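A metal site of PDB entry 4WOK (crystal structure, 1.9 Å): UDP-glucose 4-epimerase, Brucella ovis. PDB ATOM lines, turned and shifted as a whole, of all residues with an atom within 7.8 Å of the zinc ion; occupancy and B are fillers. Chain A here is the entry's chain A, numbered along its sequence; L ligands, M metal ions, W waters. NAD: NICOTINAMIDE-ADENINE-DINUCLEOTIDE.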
ATOM      1  N   PHE A  22     -22.020  11.605 -19.300  1.00  0.00           N
ATOM      2  CA  PHE A  22     -23.326  11.034 -19.633  1.00  0.00           C
ATOM      3  C   PHE A  22     -23.559  10.941 -21.155  1.00  0.00           C
ATOM      4  O   PHE A  22     -23.636   9.841 -21.735  1.00  0.00           O
ATOM      5  CB  PHE A  22     -24.405  11.879 -18.947  1.00  0.00           C
ATOM      6  CG  PHE A  22     -25.831  11.502 -19.297  1.00  0.00           C
ATOM      7  CD1 PHE A  22     -26.234  10.173 -19.330  1.00  0.00           C
ATOM      8  CD2 PHE A  22     -26.779  12.490 -19.535  1.00  0.00           C
ATOM      9  CE1 PHE A  22     -27.552   9.828 -19.651  1.00  0.00           C
ATOM     10  CE2 PHE A  22     -28.088  12.160 -19.839  1.00  0.00           C
ATOM     11  CZ  PHE A  22     -28.482  10.829 -19.893  1.00  0.00           C
ATOM     12  N   TYR A  88     -23.822  23.697 -15.803  1.00  0.00           N
ATOM     13  CA  TYR A  88     -24.861  23.933 -14.805  1.00  0.00           C
ATOM     14  C   TYR A  88     -25.224  25.405 -14.746  1.00  0.00           C
ATOM     15  O   TYR A  88     -24.395  26.273 -14.482  1.00  0.00           O
ATOM     16  CB  TYR A  88     -24.412  23.384 -13.438  1.00  0.00           C
ATOM     17  CG  TYR A  88     -24.247  21.874 -13.437  1.00  0.00           C
ATOM     18  CD1 TYR A  88     -24.731  21.109 -14.488  1.00  0.00           C
ATOM     19  CD2 TYR A  88     -23.604  21.219 -12.389  1.00  0.00           C
ATOM     20  CE1 TYR A  88     -24.587  19.740 -14.511  1.00  0.00           C
ATOM     21  CE2 TYR A  88     -23.457  19.839 -12.406  1.00  0.00           C
ATOM     22  CZ  TYR A  88     -23.960  19.112 -13.482  1.00  0.00           C
ATOM     23  OH  TYR A  88     -23.838  17.745 -13.534  1.00  0.00           O
ATOM     24  N   ALA A 181     -31.016  16.696 -21.924  1.00  0.00           N
ATOM     25  CA  ALA A 181     -30.694  15.306 -22.177  1.00  0.00           C
ATOM     26  C   ALA A 181     -31.349  14.437 -21.111  1.00  0.00           C
ATOM     27  O   ALA A 181     -31.277  14.750 -19.932  1.00  0.00           O
ATOM     28  CB  ALA A 181     -29.203  15.092 -22.148  1.00  0.00           C
ATOM     29  N   GLU A 192     -26.909   8.154 -16.164  1.00  0.00           N
ATOM     30  CA  GLU A 192     -26.514   9.525 -15.865  1.00  0.00           C
ATOM     31  C   GLU A 192     -26.057   9.598 -14.411  1.00  0.00           C
ATOM     32  O   GLU A 192     -26.890   9.475 -13.508  1.00  0.00           O
ATOM     33  CB  GLU A 192     -27.694  10.473 -16.130  1.00  0.00           C
ATOM     34  CG  GLU A 192     -27.453  11.920 -15.731  1.00  0.00           C
ATOM     35  CD  GLU A 192     -28.613  12.802 -16.153  1.00  0.00           C
ATOM     36  OE1 GLU A 192     -28.461  14.034 -16.131  1.00  0.00           O
ATOM     37  OE2 GLU A 192     -29.669  12.266 -16.534  1.00  0.00           O
ATOM     38  N   LYS A 193     -24.758   9.780 -14.178  1.00  0.00           N
ATOM     39  CA  LYS A 193     -24.244   9.780 -12.813  1.00  0.00           C
ATOM     40  C   LYS A 193     -23.569  11.108 -12.523  1.00  0.00           C
ATOM     41  O   LYS A 193     -22.398  11.340 -12.868  1.00  0.00           O
ATOM     42  CB  LYS A 193     -23.262   8.615 -12.585  1.00  0.00           C
ATOM     43  N   HIS A 194     -24.319  12.001 -11.887  1.00  0.00           N
ATOM     44  CA  HIS A 194     -23.818  13.335 -11.544  1.00  0.00           C
ATOM     45  C   HIS A 194     -23.927  13.529 -10.058  1.00  0.00           C
ATOM     46  O   HIS A 194     -24.835  12.991  -9.416  1.00  0.00           O
ATOM     47  CB  HIS A 194     -24.605  14.411 -12.286  1.00  0.00           C
ATOM     48  CG  HIS A 194     -24.432  14.391 -13.774  1.00  0.00           C
ATOM     49  ND1 HIS A 194     -25.465  14.663 -14.646  1.00  0.00           N
ATOM     50  CD2 HIS A 194     -23.352  14.137 -14.544  1.00  0.00           C
ATOM     51  CE1 HIS A 194     -25.029  14.579 -15.890  1.00  0.00           C
ATOM     52  NE2 HIS A 194     -23.745  14.268 -15.864  1.00  0.00           N
ATOM     53  N   ASP A 195     -22.988  14.274  -9.504  1.00  0.00           N
ATOM     54  CA  ASP A 195     -23.025  14.574  -8.073  1.00  0.00           C
ATOM     55  C   ASP A 195     -22.422  15.952  -7.861  1.00  0.00           C
ATOM     56  O   ASP A 195     -21.212  16.127  -7.957  1.00  0.00           O
ATOM     57  CB  ASP A 195     -22.264  13.505  -7.294  1.00  0.00           C
ATOM     58  CG  ASP A 195     -22.312  13.716  -5.792  1.00  0.00           C
ATOM     59  OD1 ASP A 195     -22.783  14.780  -5.344  1.00  0.00           O
ATOM     60  OD2 ASP A 195     -21.843  12.825  -5.058  1.00  0.00           O
ATOM     61  N   PRO A 196     -23.271  16.963  -7.568  1.00  0.00           N
ATOM     62  CA  PRO A 196     -24.711  16.843  -7.330  1.00  0.00           C
ATOM     63  C   PRO A 196     -25.498  16.621  -8.619  1.00  0.00           C
ATOM     64  O   PRO A 196     -25.094  17.066  -9.700  1.00  0.00           O
ATOM     65  CB  PRO A 196     -25.058  18.201  -6.716  1.00  0.00           C
ATOM     66  CG  PRO A 196     -24.140  19.135  -7.412  1.00  0.00           C
ATOM     67  CD  PRO A 196     -22.838  18.367  -7.581  1.00  0.00           C
ATOM     68  N   GLU A 197     -26.608  15.893  -8.497  1.00  0.00           N
ATOM     69  CA  GLU A 197     -27.491  15.695  -9.633  1.00  0.00           C
ATOM     70  C   GLU A 197     -28.492  16.850  -9.673  1.00  0.00           C
ATOM     71  O   GLU A 197     -29.272  17.004  -8.750  1.00  0.00           O
ATOM     72  CB  GLU A 197     -28.208  14.355  -9.507  1.00  0.00           C
ATOM     73  CG  GLU A 197     -29.256  14.134 -10.561  1.00  0.00           C
ATOM     74  CD  GLU A 197     -28.681  14.263 -11.953  1.00  0.00           C
ATOM     75  OE1 GLU A 197     -27.950  13.334 -12.375  1.00  0.00           O
ATOM     76  OE2 GLU A 197     -28.935  15.307 -12.599  1.00  0.00           O
ATOM     77  N   THR A 198     -28.450  17.662 -10.721  1.00  0.00           N
ATOM     78  CA  THR A 198     -29.250  18.889 -10.770  1.00  0.00           C
ATOM     79  C   THR A 198     -30.368  18.839 -11.818  1.00  0.00           C
ATOM     80  O   THR A 198     -31.150  19.778 -11.924  1.00  0.00           O
ATOM     81  CB  THR A 198     -28.368  20.125 -11.072  1.00  0.00           C
ATOM     82  OG1 THR A 198     -27.810  19.994 -12.393  1.00  0.00           O
ATOM     83  CG2 THR A 198     -27.249  20.245 -10.063  1.00  0.00           C
ATOM     84  N   HIS A 199     -30.429  17.760 -12.592  1.00  0.00           N
ATOM     85  CA  HIS A 199     -31.381  17.707 -13.696  1.00  0.00           C
ATOM     86  C   HIS A 199     -32.720  17.191 -13.205  1.00  0.00           C
ATOM     87  O   HIS A 199     -32.786  16.398 -12.266  1.00  0.00           O
ATOM     88  CB  HIS A 199     -30.819  16.838 -14.828  1.00  0.00           C
ATOM     89  CG  HIS A 199     -29.588  17.429 -15.453  1.00  0.00           C
ATOM     90  ND1 HIS A 199     -28.346  16.843 -15.340  1.00  0.00           N
ATOM     91  CD2 HIS A 199     -29.407  18.561 -16.160  1.00  0.00           C
ATOM     92  CE1 HIS A 199     -27.452  17.587 -15.960  1.00  0.00           C
ATOM     93  NE2 HIS A 199     -28.069  18.637 -16.477  1.00  0.00           N
ATOM     94  N   LEU A 200     -33.788  17.663 -13.834  1.00  0.00           N
ATOM     95  CA  LEU A 200     -35.144  17.526 -13.302  1.00  0.00           C
ATOM     96  C   LEU A 200     -35.623  16.071 -13.212  1.00  0.00           C
ATOM     97  O   LEU A 200     -36.071  15.628 -12.164  1.00  0.00           O
ATOM     98  CB  LEU A 200     -36.100  18.353 -14.173  1.00  0.00           C
ATOM     99  CG  LEU A 200     -37.547  18.558 -13.711  1.00  0.00           C
ATOM    100  CD1 LEU A 200     -38.427  17.401 -14.139  1.00  0.00           C
ATOM    101  CD2 LEU A 200     -37.613  18.799 -12.195  1.00  0.00           C
ATOM    102  N   PRO A 202     -33.946  13.144 -13.323  1.00  0.00           N
ATOM    103  CA  PRO A 202     -33.238  12.424 -12.272  1.00  0.00           C
ATOM    104  C   PRO A 202     -33.631  12.818 -10.852  1.00  0.00           C
ATOM    105  O   PRO A 202     -33.761  11.935 -10.017  1.00  0.00           O
ATOM    106  CB  PRO A 202     -31.782  12.777 -12.531  1.00  0.00           C
ATOM    107  CG  PRO A 202     -31.728  12.877 -14.030  1.00  0.00           C
ATOM    108  CD  PRO A 202     -33.006  13.604 -14.368  1.00  0.00           C
ATOM    109  N   ARG A 203     -33.790  14.113 -10.582  1.00  0.00           N
ATOM    110  CA  ARG A 203     -34.178  14.553  -9.256  1.00  0.00           C
ATOM    111  C   ARG A 203     -35.563  14.008  -8.899  1.00  0.00           C
ATOM    112  O   ARG A 203     -35.789  13.515  -7.788  1.00  0.00           O
ATOM    113  CB  ARG A 203     -34.145  16.081  -9.156  1.00  0.00           C
ATOM    114  CG  ARG A 203     -32.724  16.648  -9.076  1.00  0.00           C
ATOM    115  CD  ARG A 203     -32.718  18.168  -8.977  1.00  0.00           C
ATOM    116  NE  ARG A 203     -33.529  18.654  -7.848  1.00  0.00           N
ATOM    117  CZ  ARG A 203     -34.603  19.441  -7.979  1.00  0.00           C
ATOM    118  NH1 ARG A 203     -34.983  19.847  -9.193  1.00  0.00           N
ATOM    119  NH2 ARG A 203     -35.277  19.829  -6.906  1.00  0.00           N
ATOM    120  N   PHE A 330     -32.020   5.107 -10.856  1.00  0.00           N
ATOM    121  CA  PHE A 330     -32.230   5.965  -9.701  1.00  0.00           C
ATOM    122  C   PHE A 330     -33.059   5.270  -8.631  1.00  0.00           C
ATOM    123  O   PHE A 330     -33.828   5.909  -7.939  1.00  0.00           O
ATOM    124  CB  PHE A 330     -32.894   7.272 -10.127  1.00  0.00           C
ATOM    125  CG  PHE A 330     -32.068   8.083 -11.077  1.00  0.00           C
ATOM    126  CD1 PHE A 330     -30.947   8.780 -10.633  1.00  0.00           C
ATOM    127  CD2 PHE A 330     -32.391   8.135 -12.420  1.00  0.00           C
ATOM    128  CE1 PHE A 330     -30.165   9.510 -11.512  1.00  0.00           C
ATOM    129  CE2 PHE A 330     -31.611   8.872 -13.315  1.00  0.00           C
ATOM    130  CZ  PHE A 330     -30.502   9.558 -12.856  1.00  0.00           C
HETATM  131  PA  NAD L   1     -21.230  15.375 -18.051  1.00  0.00           P
HETATM  132  O1A NAD L   1     -20.589  16.302 -17.034  1.00  0.00           O
HETATM  133  O2A NAD L   1     -21.736  14.002 -17.745  1.00  0.00           O
HETATM  134  O5B NAD L   1     -19.971  15.095 -19.210  1.00  0.00           O
HETATM  135  C5B NAD L   1     -19.026  16.144 -19.208  1.00  0.00           C
HETATM  136  C4B NAD L   1     -17.666  15.438 -19.470  1.00  0.00           C
HETATM  137  O4B NAD L   1     -16.653  16.401 -19.778  1.00  0.00           O
HETATM  138  C3B NAD L   1     -17.329  14.776 -18.122  1.00  0.00           C
HETATM  139  O3B NAD L   1     -16.932  13.455 -18.397  1.00  0.00           O
HETATM  140  C2B NAD L   1     -16.161  15.647 -17.613  1.00  0.00           C
HETATM  141  O2B NAD L   1     -15.280  14.904 -16.862  1.00  0.00           O
HETATM  142  C1B NAD L   1     -15.502  16.092 -18.966  1.00  0.00           C
HETATM  143  N9A NAD L   1     -14.806  17.398 -18.845  1.00  0.00           N
HETATM  144  C8A NAD L   1     -15.276  18.613 -18.306  1.00  0.00           C
HETATM  145  N7A NAD L   1     -14.380  19.593 -18.392  1.00  0.00           N
HETATM  146  C5A NAD L   1     -13.276  18.987 -19.008  1.00  0.00           C
HETATM  147  C6A NAD L   1     -12.006  19.497 -19.382  1.00  0.00           C
HETATM  148  N6A NAD L   1     -11.671  20.803 -19.117  1.00  0.00           N
HETATM  149  N1A NAD L   1     -11.104  18.686 -19.984  1.00  0.00           N
HETATM  150  C2A NAD L   1     -11.478  17.382 -20.212  1.00  0.00           C
HETATM  151  N3A NAD L   1     -12.657  16.756 -19.917  1.00  0.00           N
HETATM  152  C4A NAD L   1     -13.523  17.621 -19.313  1.00  0.00           C
HETATM  153  O3  NAD L   1     -22.238  16.437 -18.738  1.00  0.00           O
HETATM  154  PN  NAD L   1     -23.166  15.877 -19.940  1.00  0.00           P
HETATM  155  O1N NAD L   1     -22.814  14.580 -20.610  1.00  0.00           O
HETATM  156  O2N NAD L   1     -24.534  16.307 -19.538  1.00  0.00           O
HETATM  157  O5D NAD L   1     -23.090  17.053 -21.205  1.00  0.00           O
HETATM  158  C5D NAD L   1     -21.870  17.176 -21.736  1.00  0.00           C
HETATM  159  C4D NAD L   1     -22.026  18.137 -22.908  1.00  0.00           C
HETATM  160  O4D NAD L   1     -23.462  18.238 -23.270  1.00  0.00           O
HETATM  161  C3D NAD L   1     -21.623  19.558 -22.449  1.00  0.00           C
HETATM  162  O3D NAD L   1     -21.102  20.178 -23.590  1.00  0.00           O
HETATM  163  C2D NAD L   1     -22.984  20.157 -22.082  1.00  0.00           C
HETATM  164  O2D NAD L   1     -23.060  21.516 -22.190  1.00  0.00           O
HETATM  165  C1D NAD L   1     -23.782  19.583 -23.270  1.00  0.00           C
HETATM  166  N1N NAD L   1     -25.293  19.750 -22.963  1.00  0.00           N
HETATM  167  C2N NAD L   1     -25.839  18.901 -22.014  1.00  0.00           C
HETATM  168  C3N NAD L   1     -27.228  19.035 -21.720  1.00  0.00           C
HETATM  169  C7N NAD L   1     -27.841  18.127 -20.682  1.00  0.00           C
HETATM  170  O7N NAD L   1     -29.042  18.190 -20.426  1.00  0.00           O
HETATM  171  N7N NAD L   1     -27.021  17.216 -20.037  1.00  0.00           N
HETATM  172  C4N NAD L   1     -27.979  20.012 -22.376  1.00  0.00           C
HETATM  173  C5N NAD L   1     -27.393  20.850 -23.322  1.00  0.00           C
HETATM  174  C6N NAD L   1     -26.031  20.707 -23.617  1.00  0.00           C
HETATM  175 ZN    ZN M   1     -27.630  15.144 -14.395  1.00  0.00          ZN
HETATM  176  O   HOH W   1     -26.285  17.380 -12.676  1.00  0.00           O
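An oxygen (O2A) of the ligand sits at hydrogen-bond distance from a ring nitrogen (NE2) of His 194, at 2.8 Å. O7N of the ligand lies within hydrogen-bond range of N of Ala 181 (2.9 Å). The backbone NH (N) of Phe 22 is in hydrogen-bond range of an oxygen (O2A) of the ligand, at 2.9 Å.
Within 4 Å of the zinc ion: Glu 192, His 194, Glu 197 and His 199. Along chain A the residues within 4 Å of the zinc ion span positions 192 to 199. The nearest printed residue that does not touch the zinc ion is Thr 198 (4.5 Å).
The zinc ion is bound by ND1 of His 199 (2.1 Å), OE1 of Glu 192 (2.2 Å), OE2 of Glu 197 (2.2 Å) and ND1 of His 194 (2.2 Å). The zinc ion has four donor atoms within binding distance. Slightly farther from the zinc ion lies the side-chain carboxylate (OE1) of Glu 197 (2.7 Å).
Water W1 lies within hydrogen-bond range of the side-chain hydroxyl (OH) of Tyr 88, the backbone NH (N) of Thr 198 and the backbone carbonyl oxygen (O) of Pro 196.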
